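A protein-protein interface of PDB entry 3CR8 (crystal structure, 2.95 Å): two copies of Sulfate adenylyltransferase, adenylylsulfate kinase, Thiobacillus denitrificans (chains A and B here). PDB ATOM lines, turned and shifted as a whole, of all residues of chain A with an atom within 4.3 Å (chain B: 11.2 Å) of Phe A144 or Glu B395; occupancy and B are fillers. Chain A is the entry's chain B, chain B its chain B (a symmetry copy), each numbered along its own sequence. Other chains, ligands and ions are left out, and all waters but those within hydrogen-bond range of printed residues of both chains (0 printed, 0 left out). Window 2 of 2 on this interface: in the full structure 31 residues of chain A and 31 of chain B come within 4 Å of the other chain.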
ATOM      1  N   PRO A 142      24.846   3.255  19.551  1.00  0.00           N
ATOM      2  CA  PRO A 142      25.894   3.997  20.247  1.00  0.00           C
ATOM      3  C   PRO A 142      25.684   5.482  20.071  1.00  0.00           C
ATOM      4  O   PRO A 142      26.064   6.277  20.917  1.00  0.00           O
ATOM      5  CB  PRO A 142      27.172   3.552  19.514  1.00  0.00           C
ATOM      6  CG  PRO A 142      26.803   2.299  18.792  1.00  0.00           C
ATOM      7  CD  PRO A 142      25.388   2.497  18.413  1.00  0.00           C
ATOM      8  N   ASP A 143      25.056   5.835  18.962  1.00  0.00           N
ATOM      9  CA  ASP A 143      24.927   7.218  18.520  1.00  0.00           C
ATOM     10  C   ASP A 143      23.664   7.899  19.036  1.00  0.00           C
ATOM     11  O   ASP A 143      22.588   7.317  19.025  1.00  0.00           O
ATOM     12  CB  ASP A 143      24.895   7.234  16.998  1.00  0.00           C
ATOM     13  CG  ASP A 143      23.858   6.262  16.424  1.00  0.00           C
ATOM     14  OD1 ASP A 143      23.944   5.023  16.664  1.00  0.00           O
ATOM     15  OD2 ASP A 143      22.948   6.759  15.729  1.00  0.00           O
ATOM     16  N   PHE A 144      23.800   9.137  19.485  1.00  0.00           N
ATOM     17  CA  PHE A 144      22.663   9.954  19.879  1.00  0.00           C
ATOM     18  C   PHE A 144      21.902   9.354  21.067  1.00  0.00           C
ATOM     19  O   PHE A 144      20.683   9.513  21.217  1.00  0.00           O
ATOM     20  CB  PHE A 144      21.757  10.241  18.676  1.00  0.00           C
ATOM     21  CG  PHE A 144      22.448  10.965  17.564  1.00  0.00           C
ATOM     22  CD1 PHE A 144      23.387  11.941  17.846  1.00  0.00           C
ATOM     23  CD2 PHE A 144      22.171  10.677  16.248  1.00  0.00           C
ATOM     24  CE1 PHE A 144      24.059  12.603  16.833  1.00  0.00           C
ATOM     25  CE2 PHE A 144      22.813  11.336  15.228  1.00  0.00           C
ATOM     26  CZ  PHE A 144      23.761  12.300  15.517  1.00  0.00           C
ATOM     27  N   VAL A 145      22.647   8.692  21.939  1.00  0.00           N
ATOM     28  CA  VAL A 145      22.064   8.146  23.151  1.00  0.00           C
ATOM     29  C   VAL A 145      21.105   9.111  23.855  1.00  0.00           C
ATOM     30  O   VAL A 145      19.978   8.748  24.172  1.00  0.00           O
ATOM     31  CB  VAL A 145      23.153   7.607  24.084  1.00  0.00           C
ATOM     32  CG1 VAL A 145      22.846   7.907  25.546  1.00  0.00           C
ATOM     33  CG2 VAL A 145      23.303   6.110  23.857  1.00  0.00           C
ATOM     34  N   SER A 146      21.533  10.341  24.097  1.00  0.00           N
ATOM     35  CA  SER A 146      20.640  11.342  24.698  1.00  0.00           C
ATOM     36  C   SER A 146      19.306  11.425  23.965  1.00  0.00           C
ATOM     37  O   SER A 146      18.247  11.178  24.550  1.00  0.00           O
ATOM     38  CB  SER A 146      21.300  12.710  24.662  1.00  0.00           C
ATOM     39  OG  SER A 146      22.161  12.813  23.531  1.00  0.00           O
ATOM     40  N   LEU A 147      19.383  11.731  22.671  1.00  0.00           N
ATOM     41  CA  LEU A 147      18.234  12.039  21.822  1.00  0.00           C
ATOM     42  C   LEU A 147      17.244  10.920  21.579  1.00  0.00           C
ATOM     43  O   LEU A 147      16.113  11.174  21.147  1.00  0.00           O
ATOM     44  CB  LEU A 147      18.721  12.549  20.479  1.00  0.00           C
ATOM     45  CG  LEU A 147      19.318  13.939  20.667  1.00  0.00           C
ATOM     46  CD1 LEU A 147      20.070  14.360  19.412  1.00  0.00           C
ATOM     47  CD2 LEU A 147      18.195  14.967  21.084  1.00  0.00           C
ATOM     48  N   ARG A 148      17.655   9.688  21.848  1.00  0.00           N
ATOM     49  CA  ARG A 148      16.761   8.541  21.681  1.00  0.00           C
ATOM     50  C   ARG A 148      15.909   8.219  22.916  1.00  0.00           C
ATOM     51  O   ARG A 148      16.417   7.724  23.936  1.00  0.00           O
ATOM     52  CB  ARG A 148      17.575   7.307  21.304  1.00  0.00           C
ATOM     53  CG  ARG A 148      18.417   7.505  20.052  1.00  0.00           C
ATOM     54  CD  ARG A 148      19.441   6.387  19.860  1.00  0.00           C
ATOM     55  NE  ARG A 148      20.027   6.416  18.526  1.00  0.00           N
ATOM     56  CZ  ARG A 148      19.404   5.961  17.442  1.00  0.00           C
ATOM     57  NH1 ARG A 148      18.180   5.449  17.545  1.00  0.00           N
ATOM     58  NH2 ARG A 148      19.995   6.015  16.257  1.00  0.00           N
ATOM     59  N   PHE A 211      22.295  10.503  10.080  1.00  0.00           N
ATOM     60  CA  PHE A 211      23.229  11.343  10.812  1.00  0.00           C
ATOM     61  C   PHE A 211      23.098  12.805  10.383  1.00  0.00           C
ATOM     62  O   PHE A 211      22.915  13.686  11.214  1.00  0.00           O
ATOM     63  CB  PHE A 211      24.655  10.834  10.652  1.00  0.00           C
ATOM     64  CG  PHE A 211      24.961   9.621  11.481  1.00  0.00           C
ATOM     65  CD1 PHE A 211      25.480   9.749  12.757  1.00  0.00           C
ATOM     66  CD2 PHE A 211      24.731   8.362  10.984  1.00  0.00           C
ATOM     67  CE1 PHE A 211      25.751   8.653  13.517  1.00  0.00           C
ATOM     68  CE2 PHE A 211      25.010   7.262  11.746  1.00  0.00           C
ATOM     69  CZ  PHE A 211      25.511   7.413  13.021  1.00  0.00           C
ATOM     70  N   VAL A 214      19.816  14.277  11.658  1.00  0.00           N
ATOM     71  CA  VAL A 214      19.873  14.633  13.063  1.00  0.00           C
ATOM     72  C   VAL A 214      20.681  15.891  13.237  1.00  0.00           C
ATOM     73  O   VAL A 214      20.292  16.785  13.987  1.00  0.00           O
ATOM     74  CB  VAL A 214      20.478  13.533  13.919  1.00  0.00           C
ATOM     75  CG1 VAL A 214      20.693  14.019  15.356  1.00  0.00           C
ATOM     76  CG2 VAL A 214      19.575  12.362  13.909  1.00  0.00           C
ATOM     77  N   ARG A 215      21.808  15.975  12.542  1.00  0.00           N
ATOM     78  CA  ARG A 215      22.681  17.145  12.695  1.00  0.00           C
ATOM     79  C   ARG A 215      22.051  18.468  12.188  1.00  0.00           C
ATOM     80  O   ARG A 215      22.285  19.532  12.740  1.00  0.00           O
ATOM     81  CB  ARG A 215      24.060  16.891  12.083  1.00  0.00           C
ATOM     82  CG  ARG A 215      25.203  17.489  12.911  1.00  0.00           C
ATOM     83  CD  ARG A 215      26.429  16.671  12.717  1.00  0.00           C
ATOM     84  NE  ARG A 215      26.403  16.114  11.376  1.00  0.00           N
ATOM     85  CZ  ARG A 215      26.865  14.908  11.067  1.00  0.00           C
ATOM     86  NH1 ARG A 215      27.400  14.145  12.028  1.00  0.00           N
ATOM     87  NH2 ARG A 215      26.785  14.461   9.807  1.00  0.00           N
ATOM     88  N   LEU A 233      14.450  11.453  18.878  1.00  0.00           N
ATOM     89  CA  LEU A 233      14.534  10.652  17.668  1.00  0.00           C
ATOM     90  C   LEU A 233      13.489   9.561  17.625  1.00  0.00           C
ATOM     91  O   LEU A 233      13.169   8.937  18.642  1.00  0.00           O
ATOM     92  CB  LEU A 233      15.923  10.059  17.521  1.00  0.00           C
ATOM     93  CG  LEU A 233      16.953  11.172  17.652  1.00  0.00           C
ATOM     94  CD1 LEU A 233      18.347  10.622  17.595  1.00  0.00           C
ATOM     95  CD2 LEU A 233      16.717  12.141  16.547  1.00  0.00           C
ATOM     96  N   PHE B 370      42.379  10.487  10.365  1.00  0.00           N
ATOM     97  CA  PHE B 370      43.067   9.531  11.197  1.00  0.00           C
ATOM     98  C   PHE B 370      42.380   8.225  11.017  1.00  0.00           C
ATOM     99  O   PHE B 370      41.179   8.201  10.718  1.00  0.00           O
ATOM    100  CB  PHE B 370      43.078   9.958  12.679  1.00  0.00           C
ATOM    101  CG  PHE B 370      41.704  10.142  13.300  1.00  0.00           C
ATOM    102  CD1 PHE B 370      40.986  11.306  13.107  1.00  0.00           C
ATOM    103  CD2 PHE B 370      41.145   9.152  14.104  1.00  0.00           C
ATOM    104  CE1 PHE B 370      39.714  11.465  13.680  1.00  0.00           C
ATOM    105  CE2 PHE B 370      39.874   9.307  14.690  1.00  0.00           C
ATOM    106  CZ  PHE B 370      39.161  10.462  14.473  1.00  0.00           C
ATOM    107  N   ARG B 387      32.510  -1.277  15.012  1.00  0.00           N
ATOM    108  CA  ARG B 387      31.180  -0.773  14.645  1.00  0.00           C
ATOM    109  C   ARG B 387      30.611   0.267  15.609  1.00  0.00           C
ATOM    110  O   ARG B 387      30.076   1.266  15.167  1.00  0.00           O
ATOM    111  CB  ARG B 387      30.164  -1.905  14.501  1.00  0.00           C
ATOM    112  CG  ARG B 387      29.906  -2.325  13.077  1.00  0.00           C
ATOM    113  CD  ARG B 387      28.802  -3.346  12.998  1.00  0.00           C
ATOM    114  NE  ARG B 387      27.478  -2.726  12.956  1.00  0.00           N
ATOM    115  CZ  ARG B 387      26.860  -2.392  11.826  1.00  0.00           C
ATOM    116  NH1 ARG B 387      27.469  -2.624  10.661  1.00  0.00           N
ATOM    117  NH2 ARG B 387      25.650  -1.827  11.856  1.00  0.00           N
ATOM    118  N   ALA B 388      30.691   0.032  16.913  1.00  0.00           N
ATOM    119  CA  ALA B 388      30.098   0.974  17.841  1.00  0.00           C
ATOM    120  C   ALA B 388      30.838   2.314  17.734  1.00  0.00           C
ATOM    121  O   ALA B 388      30.223   3.399  17.760  1.00  0.00           O
ATOM    122  CB  ALA B 388      30.127   0.415  19.272  1.00  0.00           C
ATOM    123  N   LEU B 389      32.160   2.229  17.590  1.00  0.00           N
ATOM    124  CA  LEU B 389      32.991   3.413  17.601  1.00  0.00           C
ATOM    125  C   LEU B 389      32.682   4.232  16.356  1.00  0.00           C
ATOM    126  O   LEU B 389      32.615   5.455  16.415  1.00  0.00           O
ATOM    127  CB  LEU B 389      34.444   3.015  17.673  1.00  0.00           C
ATOM    128  CG  LEU B 389      35.527   4.058  18.008  1.00  0.00           C
ATOM    129  CD1 LEU B 389      36.538   4.236  16.869  1.00  0.00           C
ATOM    130  CD2 LEU B 389      34.953   5.389  18.471  1.00  0.00           C
ATOM    131  N   ALA B 390      32.461   3.551  15.235  1.00  0.00           N
ATOM    132  CA  ALA B 390      31.990   4.202  14.010  1.00  0.00           C
ATOM    133  C   ALA B 390      30.699   4.978  14.237  1.00  0.00           C
ATOM    134  O   ALA B 390      30.587   6.110  13.809  1.00  0.00           O
ATOM    135  CB  ALA B 390      31.781   3.184  12.919  1.00  0.00           C
ATOM    136  N   ALA B 391      29.716   4.359  14.883  1.00  0.00           N
ATOM    137  CA  ALA B 391      28.440   5.011  15.073  1.00  0.00           C
ATOM    138  C   ALA B 391      28.659   6.315  15.823  1.00  0.00           C
ATOM    139  O   ALA B 391      28.151   7.352  15.399  1.00  0.00           O
ATOM    140  CB  ALA B 391      27.453   4.092  15.808  1.00  0.00           C
ATOM    141  N   ARG B 392      29.420   6.265  16.925  1.00  0.00           N
ATOM    142  CA  ARG B 392      29.678   7.458  17.770  1.00  0.00           C
ATOM    143  C   ARG B 392      30.324   8.578  16.964  1.00  0.00           C
ATOM    144  O   ARG B 392      29.824   9.698  16.936  1.00  0.00           O
ATOM    145  CB  ARG B 392      30.596   7.137  18.948  1.00  0.00           C
ATOM    146  CG  ARG B 392      30.014   6.254  20.001  1.00  0.00           C
ATOM    147  CD  ARG B 392      28.846   6.936  20.694  1.00  0.00           C
ATOM    148  NE  ARG B 392      29.030   8.376  20.780  1.00  0.00           N
ATOM    149  CZ  ARG B 392      29.392   9.009  21.886  1.00  0.00           C
ATOM    150  NH1 ARG B 392      29.620   8.329  23.007  1.00  0.00           N
ATOM    151  NH2 ARG B 392      29.529  10.325  21.864  1.00  0.00           N
ATOM    152  N   LEU B 393      31.437   8.249  16.307  1.00  0.00           N
ATOM    153  CA  LEU B 393      32.154   9.193  15.466  1.00  0.00           C
ATOM    154  C   LEU B 393      31.317   9.807  14.351  1.00  0.00           C
ATOM    155  O   LEU B 393      31.625  10.889  13.873  1.00  0.00           O
ATOM    156  CB  LEU B 393      33.399   8.555  14.869  1.00  0.00           C
ATOM    157  CG  LEU B 393      34.412   8.239  15.957  1.00  0.00           C
ATOM    158  CD1 LEU B 393      35.731   7.728  15.395  1.00  0.00           C
ATOM    159  CD2 LEU B 393      34.649   9.444  16.830  1.00  0.00           C
ATOM    160  N   MET B 394      30.263   9.127  13.938  1.00  0.00           N
ATOM    161  CA  MET B 394      29.373   9.648  12.904  1.00  0.00           C
ATOM    162  C   MET B 394      28.466  10.773  13.408  1.00  0.00           C
ATOM    163  O   MET B 394      28.006  11.590  12.603  1.00  0.00           O
ATOM    164  CB  MET B 394      28.528   8.521  12.291  1.00  0.00           C
ATOM    165  CG  MET B 394      29.354   7.554  11.421  1.00  0.00           C
ATOM    166  SD  MET B 394      28.441   6.438  10.325  1.00  0.00           S
ATOM    167  CE  MET B 394      29.842   5.739   9.479  1.00  0.00           C
ATOM    168  N   GLU B 395      28.222  10.814  14.724  1.00  0.00           N
ATOM    169  CA  GLU B 395      27.498  11.917  15.333  1.00  0.00           C
ATOM    170  C   GLU B 395      28.154  13.295  15.052  1.00  0.00           C
ATOM    171  O   GLU B 395      27.549  14.350  15.226  1.00  0.00           O
ATOM    172  CB  GLU B 395      27.418  11.726  16.849  1.00  0.00           C
ATOM    173  CG  GLU B 395      26.559  10.584  17.359  1.00  0.00           C
ATOM    174  CD  GLU B 395      26.410  10.610  18.884  1.00  0.00           C
ATOM    175  OE1 GLU B 395      26.057   9.554  19.469  1.00  0.00           O
ATOM    176  OE2 GLU B 395      26.640  11.685  19.496  1.00  0.00           O
ATOM    177  N   MET B 396      29.399  13.293  14.618  1.00  0.00           N
ATOM    178  CA  MET B 396      30.171  14.527  14.611  1.00  0.00           C
ATOM    179  C   MET B 396      30.132  15.328  13.332  1.00  0.00           C
ATOM    180  O   MET B 396      30.147  16.555  13.382  1.00  0.00           O
ATOM    181  CB  MET B 396      31.615  14.273  15.021  1.00  0.00           C
ATOM    182  CG  MET B 396      31.717  13.847  16.476  1.00  0.00           C
ATOM    183  SD  MET B 396      33.385  13.451  16.996  1.00  0.00           S
ATOM    184  CE  MET B 396      33.076  12.950  18.706  1.00  0.00           C
ATOM    185  N   GLY B 397      30.087  14.671  12.184  1.00  0.00           N
ATOM    186  CA  GLY B 397      30.081  15.422  10.940  1.00  0.00           C
ATOM    187  C   GLY B 397      31.411  16.141  10.751  1.00  0.00           C
ATOM    188  O   GLY B 397      32.322  16.051  11.600  1.00  0.00           O
ATOM    189  N   GLY B 398      31.549  16.843   9.632  1.00  0.00           N
ATOM    190  CA  GLY B 398      32.830  17.438   9.320  1.00  0.00           C
ATOM    191  C   GLY B 398      33.771  16.436   8.680  1.00  0.00           C
ATOM    192  O   GLY B 398      34.243  16.658   7.568  1.00  0.00           O
ATOM    193  N   ARG B 399      34.065  15.340   9.369  1.00  0.00           N
ATOM    194  CA  ARG B 399      34.827  14.259   8.727  1.00  0.00           C
ATOM    195  C   ARG B 399      33.940  13.045   8.485  1.00  0.00           C
ATOM    196  O   ARG B 399      33.109  12.701   9.342  1.00  0.00           O
ATOM    197  CB  ARG B 399      36.065  13.883   9.551  1.00  0.00           C
ATOM    198  CG  ARG B 399      37.090  15.007   9.587  1.00  0.00           C
ATOM    199  CD  ARG B 399      38.133  14.819  10.643  1.00  0.00           C
ATOM    200  NE  ARG B 399      37.544  14.784  11.976  1.00  0.00           N
ATOM    201  CZ  ARG B 399      38.246  14.795  13.107  1.00  0.00           C
ATOM    202  NH1 ARG B 399      39.562  14.841  13.084  1.00  0.00           N
ATOM    203  NH2 ARG B 399      37.632  14.745  14.267  1.00  0.00           N
ATOM    204  N   CYS B 400      34.095  12.418   7.318  1.00  0.00           N
ATOM    205  CA  CYS B 400      33.341  11.206   6.983  1.00  0.00           C
ATOM    206  C   CYS B 400      33.982   9.958   7.582  1.00  0.00           C
ATOM    207  O   CYS B 400      35.198   9.847   7.626  1.00  0.00           O
ATOM    208  CB  CYS B 400      33.155  11.055   5.469  1.00  0.00           C
ATOM    209  SG  CYS B 400      32.076  12.319   4.769  1.00  0.00           S
ATOM    210  N   VAL B 401      33.161   9.034   8.080  1.00  0.00           N
ATOM    211  CA  VAL B 401      33.678   7.809   8.686  1.00  0.00           C
ATOM    212  C   VAL B 401      33.425   6.602   7.782  1.00  0.00           C
ATOM    213  O   VAL B 401      32.328   6.415   7.264  1.00  0.00           O
ATOM    214  CB  VAL B 401      33.054   7.534  10.058  1.00  0.00           C
ATOM    215  CG1 VAL B 401      33.654   6.262  10.649  1.00  0.00           C
ATOM    216  CG2 VAL B 401      33.239   8.733  10.979  1.00  0.00           C
ATOM    217  N   THR B 402      34.457   5.792   7.589  1.00  0.00           N
ATOM    218  CA  THR B 402      34.328   4.550   6.835  1.00  0.00           C
ATOM    219  C   THR B 402      34.761   3.337   7.663  1.00  0.00           C
ATOM    220  O   THR B 402      35.852   3.310   8.221  1.00  0.00           O
ATOM    221  CB  THR B 402      35.175   4.563   5.571  1.00  0.00           C
ATOM    222  OG1 THR B 402      34.652   5.525   4.649  1.00  0.00           O
ATOM    223  CG2 THR B 402      35.146   3.181   4.942  1.00  0.00           C
ATOM    224  N   ILE B 444      37.950   9.781   8.547  1.00  0.00           N
ATOM    225  CA  ILE B 444      38.433   8.874   9.574  1.00  0.00           C
ATOM    226  C   ILE B 444      38.153   7.445   9.139  1.00  0.00           C
ATOM    227  O   ILE B 444      37.026   7.125   8.775  1.00  0.00           O
ATOM    228  CB  ILE B 444      37.918   9.178  11.020  1.00  0.00           C
ATOM    229  CG1 ILE B 444      36.832   8.224  11.437  1.00  0.00           C
ATOM    230  CG2 ILE B 444      37.430  10.601  11.206  1.00  0.00           C
ATOM    231  CD1 ILE B 444      36.233   8.640  12.738  1.00  0.00           C
ATOM    232  N   ILE B 446      38.250   3.304  10.105  1.00  0.00           N
ATOM    233  CA  ILE B 446      38.255   2.411  11.254  1.00  0.00           C
ATOM    234  C   ILE B 446      38.418   0.979  10.808  1.00  0.00           C
ATOM    235  O   ILE B 446      37.537   0.415  10.149  1.00  0.00           O
ATOM    236  CB  ILE B 446      36.938   2.509  12.038  1.00  0.00           C
ATOM    237  CG1 ILE B 446      36.785   3.907  12.641  1.00  0.00           C
ATOM    238  CG2 ILE B 446      36.836   1.386  13.088  1.00  0.00           C
ATOM    239  CD1 ILE B 446      35.343   4.227  12.947  1.00  0.00           C
ATOM    240  N   ASP B 527      29.611  -0.119  25.695  1.00  0.00           N
ATOM    241  CA  ASP B 527      29.534   1.285  26.052  1.00  0.00           C
ATOM    242  C   ASP B 527      30.796   1.759  26.772  1.00  0.00           C
ATOM    243  O   ASP B 527      31.420   2.730  26.342  1.00  0.00           O
ATOM    244  CB  ASP B 527      28.303   1.535  26.906  1.00  0.00           C
ATOM    245  CG  ASP B 527      27.029   1.522  26.093  1.00  0.00           C
ATOM    246  OD1 ASP B 527      27.140   1.407  24.868  1.00  0.00           O
ATOM    247  OD2 ASP B 527      25.920   1.639  26.667  1.00  0.00           O
ATOM    248  N   VAL B 530      33.899   1.728  24.411  1.00  0.00           N
ATOM    249  CA  VAL B 530      33.759   2.808  23.436  1.00  0.00           C
ATOM    250  C   VAL B 530      34.107   4.174  24.036  1.00  0.00           C
ATOM    251  O   VAL B 530      34.851   4.951  23.449  1.00  0.00           O
ATOM    252  CB  VAL B 530      32.330   2.879  22.889  1.00  0.00           C
ATOM    253  CG1 VAL B 530      32.074   4.215  22.214  1.00  0.00           C
ATOM    254  CG2 VAL B 530      32.106   1.772  21.907  1.00  0.00           C
ATOM    255  N   GLN B 531      33.574   4.447  25.216  1.00  0.00           N
ATOM    256  CA  GLN B 531      33.845   5.694  25.924  1.00  0.00           C
ATOM    257  C   GLN B 531      35.317   5.809  26.204  1.00  0.00           C
ATOM    258  O   GLN B 531      35.910   6.864  25.985  1.00  0.00           O
ATOM    259  CB  GLN B 531      33.090   5.717  27.252  1.00  0.00           C
ATOM    260  CG  GLN B 531      33.184   7.013  27.971  1.00  0.00           C
ATOM    261  CD  GLN B 531      32.772   8.165  27.094  1.00  0.00           C
ATOM    262  OE1 GLN B 531      31.922   8.016  26.193  1.00  0.00           O
ATOM    263  NE2 GLN B 531      33.360   9.336  27.348  1.00  0.00           N
ATOM    264  N   LEU B 534      36.872   7.021  23.230  1.00  0.00           N
ATOM    265  CA  LEU B 534      36.584   8.410  22.883  1.00  0.00           C
ATOM    266  C   LEU B 534      37.471   9.260  23.768  1.00  0.00           C
ATOM    267  O   LEU B 534      37.955  10.311  23.358  1.00  0.00           O
ATOM    268  CB  LEU B 534      35.110   8.765  23.014  1.00  0.00           C
ATOM    269  CG  LEU B 534      34.286   8.093  21.918  1.00  0.00           C
ATOM    270  CD1 LEU B 534      32.795   8.066  22.273  1.00  0.00           C
ATOM    271  CD2 LEU B 534      34.542   8.738  20.567  1.00  0.00           C
ATOM    272  N   LEU B 537      40.863   9.404  21.919  1.00  0.00           N
ATOM    273  CA  LEU B 537      40.793  10.438  20.887  1.00  0.00           C
ATOM    274  C   LEU B 537      40.681  11.889  21.435  1.00  0.00           C
ATOM    275  O   LEU B 537      41.338  12.813  20.936  1.00  0.00           O
ATOM    276  CB  LEU B 537      39.651  10.138  19.903  1.00  0.00           C
ATOM    277  CG  LEU B 537      39.674   8.722  19.318  1.00  0.00           C
ATOM    278  CD1 LEU B 537      38.379   8.354  18.604  1.00  0.00           C
ATOM    279  CD2 LEU B 537      40.857   8.554  18.384  1.00  0.00           C
ATOM    280  N   LEU B 543      39.361  14.970  18.305  1.00  0.00           N
ATOM    281  CA  LEU B 543      37.930  15.305  18.325  1.00  0.00           C
ATOM    282  C   LEU B 543      37.701  16.827  18.313  1.00  0.00           C
ATOM    283  O   LEU B 543      38.523  17.578  18.840  1.00  0.00           O
ATOM    284  CB  LEU B 543      37.240  14.672  19.537  1.00  0.00           C
ATOM    285  CG  LEU B 543      37.278  13.155  19.530  1.00  0.00           C
ATOM    286  CD1 LEU B 543      36.387  12.652  20.638  1.00  0.00           C
ATOM    287  CD2 LEU B 543      36.827  12.651  18.165  1.00  0.00           C
ATOM    288  N   ARG B 544      36.661  17.273  17.628  1.00  0.00           N
ATOM    289  CA  ARG B 544      36.472  18.685  17.386  1.00  0.00           C
ATOM    290  C   ARG B 544      35.498  19.287  18.370  1.00  0.00           C
ATOM    291  O   ARG B 544      34.299  19.127  18.232  1.00  0.00           O
ATOM    292  CB  ARG B 544      35.982  18.912  15.959  1.00  0.00           C
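NH1 of Arg A215 sits at hydrogen-bond distance from O of Glu B395 (3.2 Å).
The guanidinium group (NH1) of Arg A215 lies close to the backbone NH (N) of Gly B397 (2.7 Å).
NH1 of Arg A215 is in hydrogen-bond range of O of Met B394 (2.7 Å).
NH1 of Arg A215 lies close to N of Met B396, at 3.4 Å.
OE1 of Glu B395 lies close to N of Phe A144 (2.3 Å).
Of the 11 printed residues of chain A, 5 touch a printed residue of chain B.
Printed residues of chain A that touch a printed residue of chain B: Pro A142, Asp A143, Phe A144, Phe A211 and Arg A215.
Along chain A the printed residues that touch a printed residue of chain B span positions 142 to 215.
Among the printed residues, no Asp or Glu carboxylate lies within 4 Å of a Lys or Arg side-chain nitrogen of the other chain.
No position is printed for both chains.
Of the printed residues of chain B, Pro A142 touches Ala B388 (3.5 Å), Ala B391 (3.5 Å), Arg B392 (2.9 Å) and Glu B395 (3.6 Å).
Asp A143 touches two residues of chain B.
Phe A144 touches one residue of chain B.
No residue of chain B comes within 4 Å of Val A145.
No residue of chain B comes within 4 Å of Ser A146.
No residue of chain B comes within 4 Å of Leu A147.
Arg A148 touches none of the printed residues of chain B.
Of chain B, only Ala B391 (3.3 Å), Met B394 (3.0 Å) and Glu B395 (3.5 Å) come within 4 Å of Phe A211.
No residue of chain B comes within 4 Å of Val A214.
Of the printed residues of chain B, Arg A215 touches Met B394, Glu B395, Met B396 and Gly B397.
Of the printed residues of chain A, Ala B388 touches Pro A142.
Of the printed residues of chain A, Arg B392 touches Pro A142 (2.9 Å).
Printed residues of chain A within 4 Å of Met B394: Phe A211 and Arg A215.
Of the printed residues of chain A, Glu B395 touches Pro A142, Asp A143, Phe A144, Phe A211 and Arg A215.
Gln B531 touches none of the printed residues of chain A.
Leu B534 touches none of the printed residues of chain A.
The nearest printed residue of chain A that does not touch Glu B395 is Val A145 (4.3 Å).
The nearest printed residue of chain A that does not touch Ala B388 is Asp A143 (5.8 Å).
CB of Pro A142 touches O of Ala B388, at 3.5 Å.
Pro A142 touches Ala B391 (CG to CB, 3.5 Å).
Pro A142 touches Arg B392 (O to CD, 2.9 Å).
Pro A142 touches Glu B395 (O to OE1, 3.6 Å).
Ala B391 touches Asp A143 (O to CB, 3.6 Å).
CA of Asp A143 touches OE1 of Glu B395, at 2.8 Å.
Ala B391 touches Phe A211.
CB of Met B394 touches CE1 of Phe A211, 3.0 Å away.
Glu B395 touches Phe A211.
OD2 of Asp A143 is in salt-bridge range of NH2 of Arg A148, 3.1 Å away.
The side-chain carboxylate of Glu B395 lies within salt-bridge range of the guanidinium group of Arg B392 (3.5 Å).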
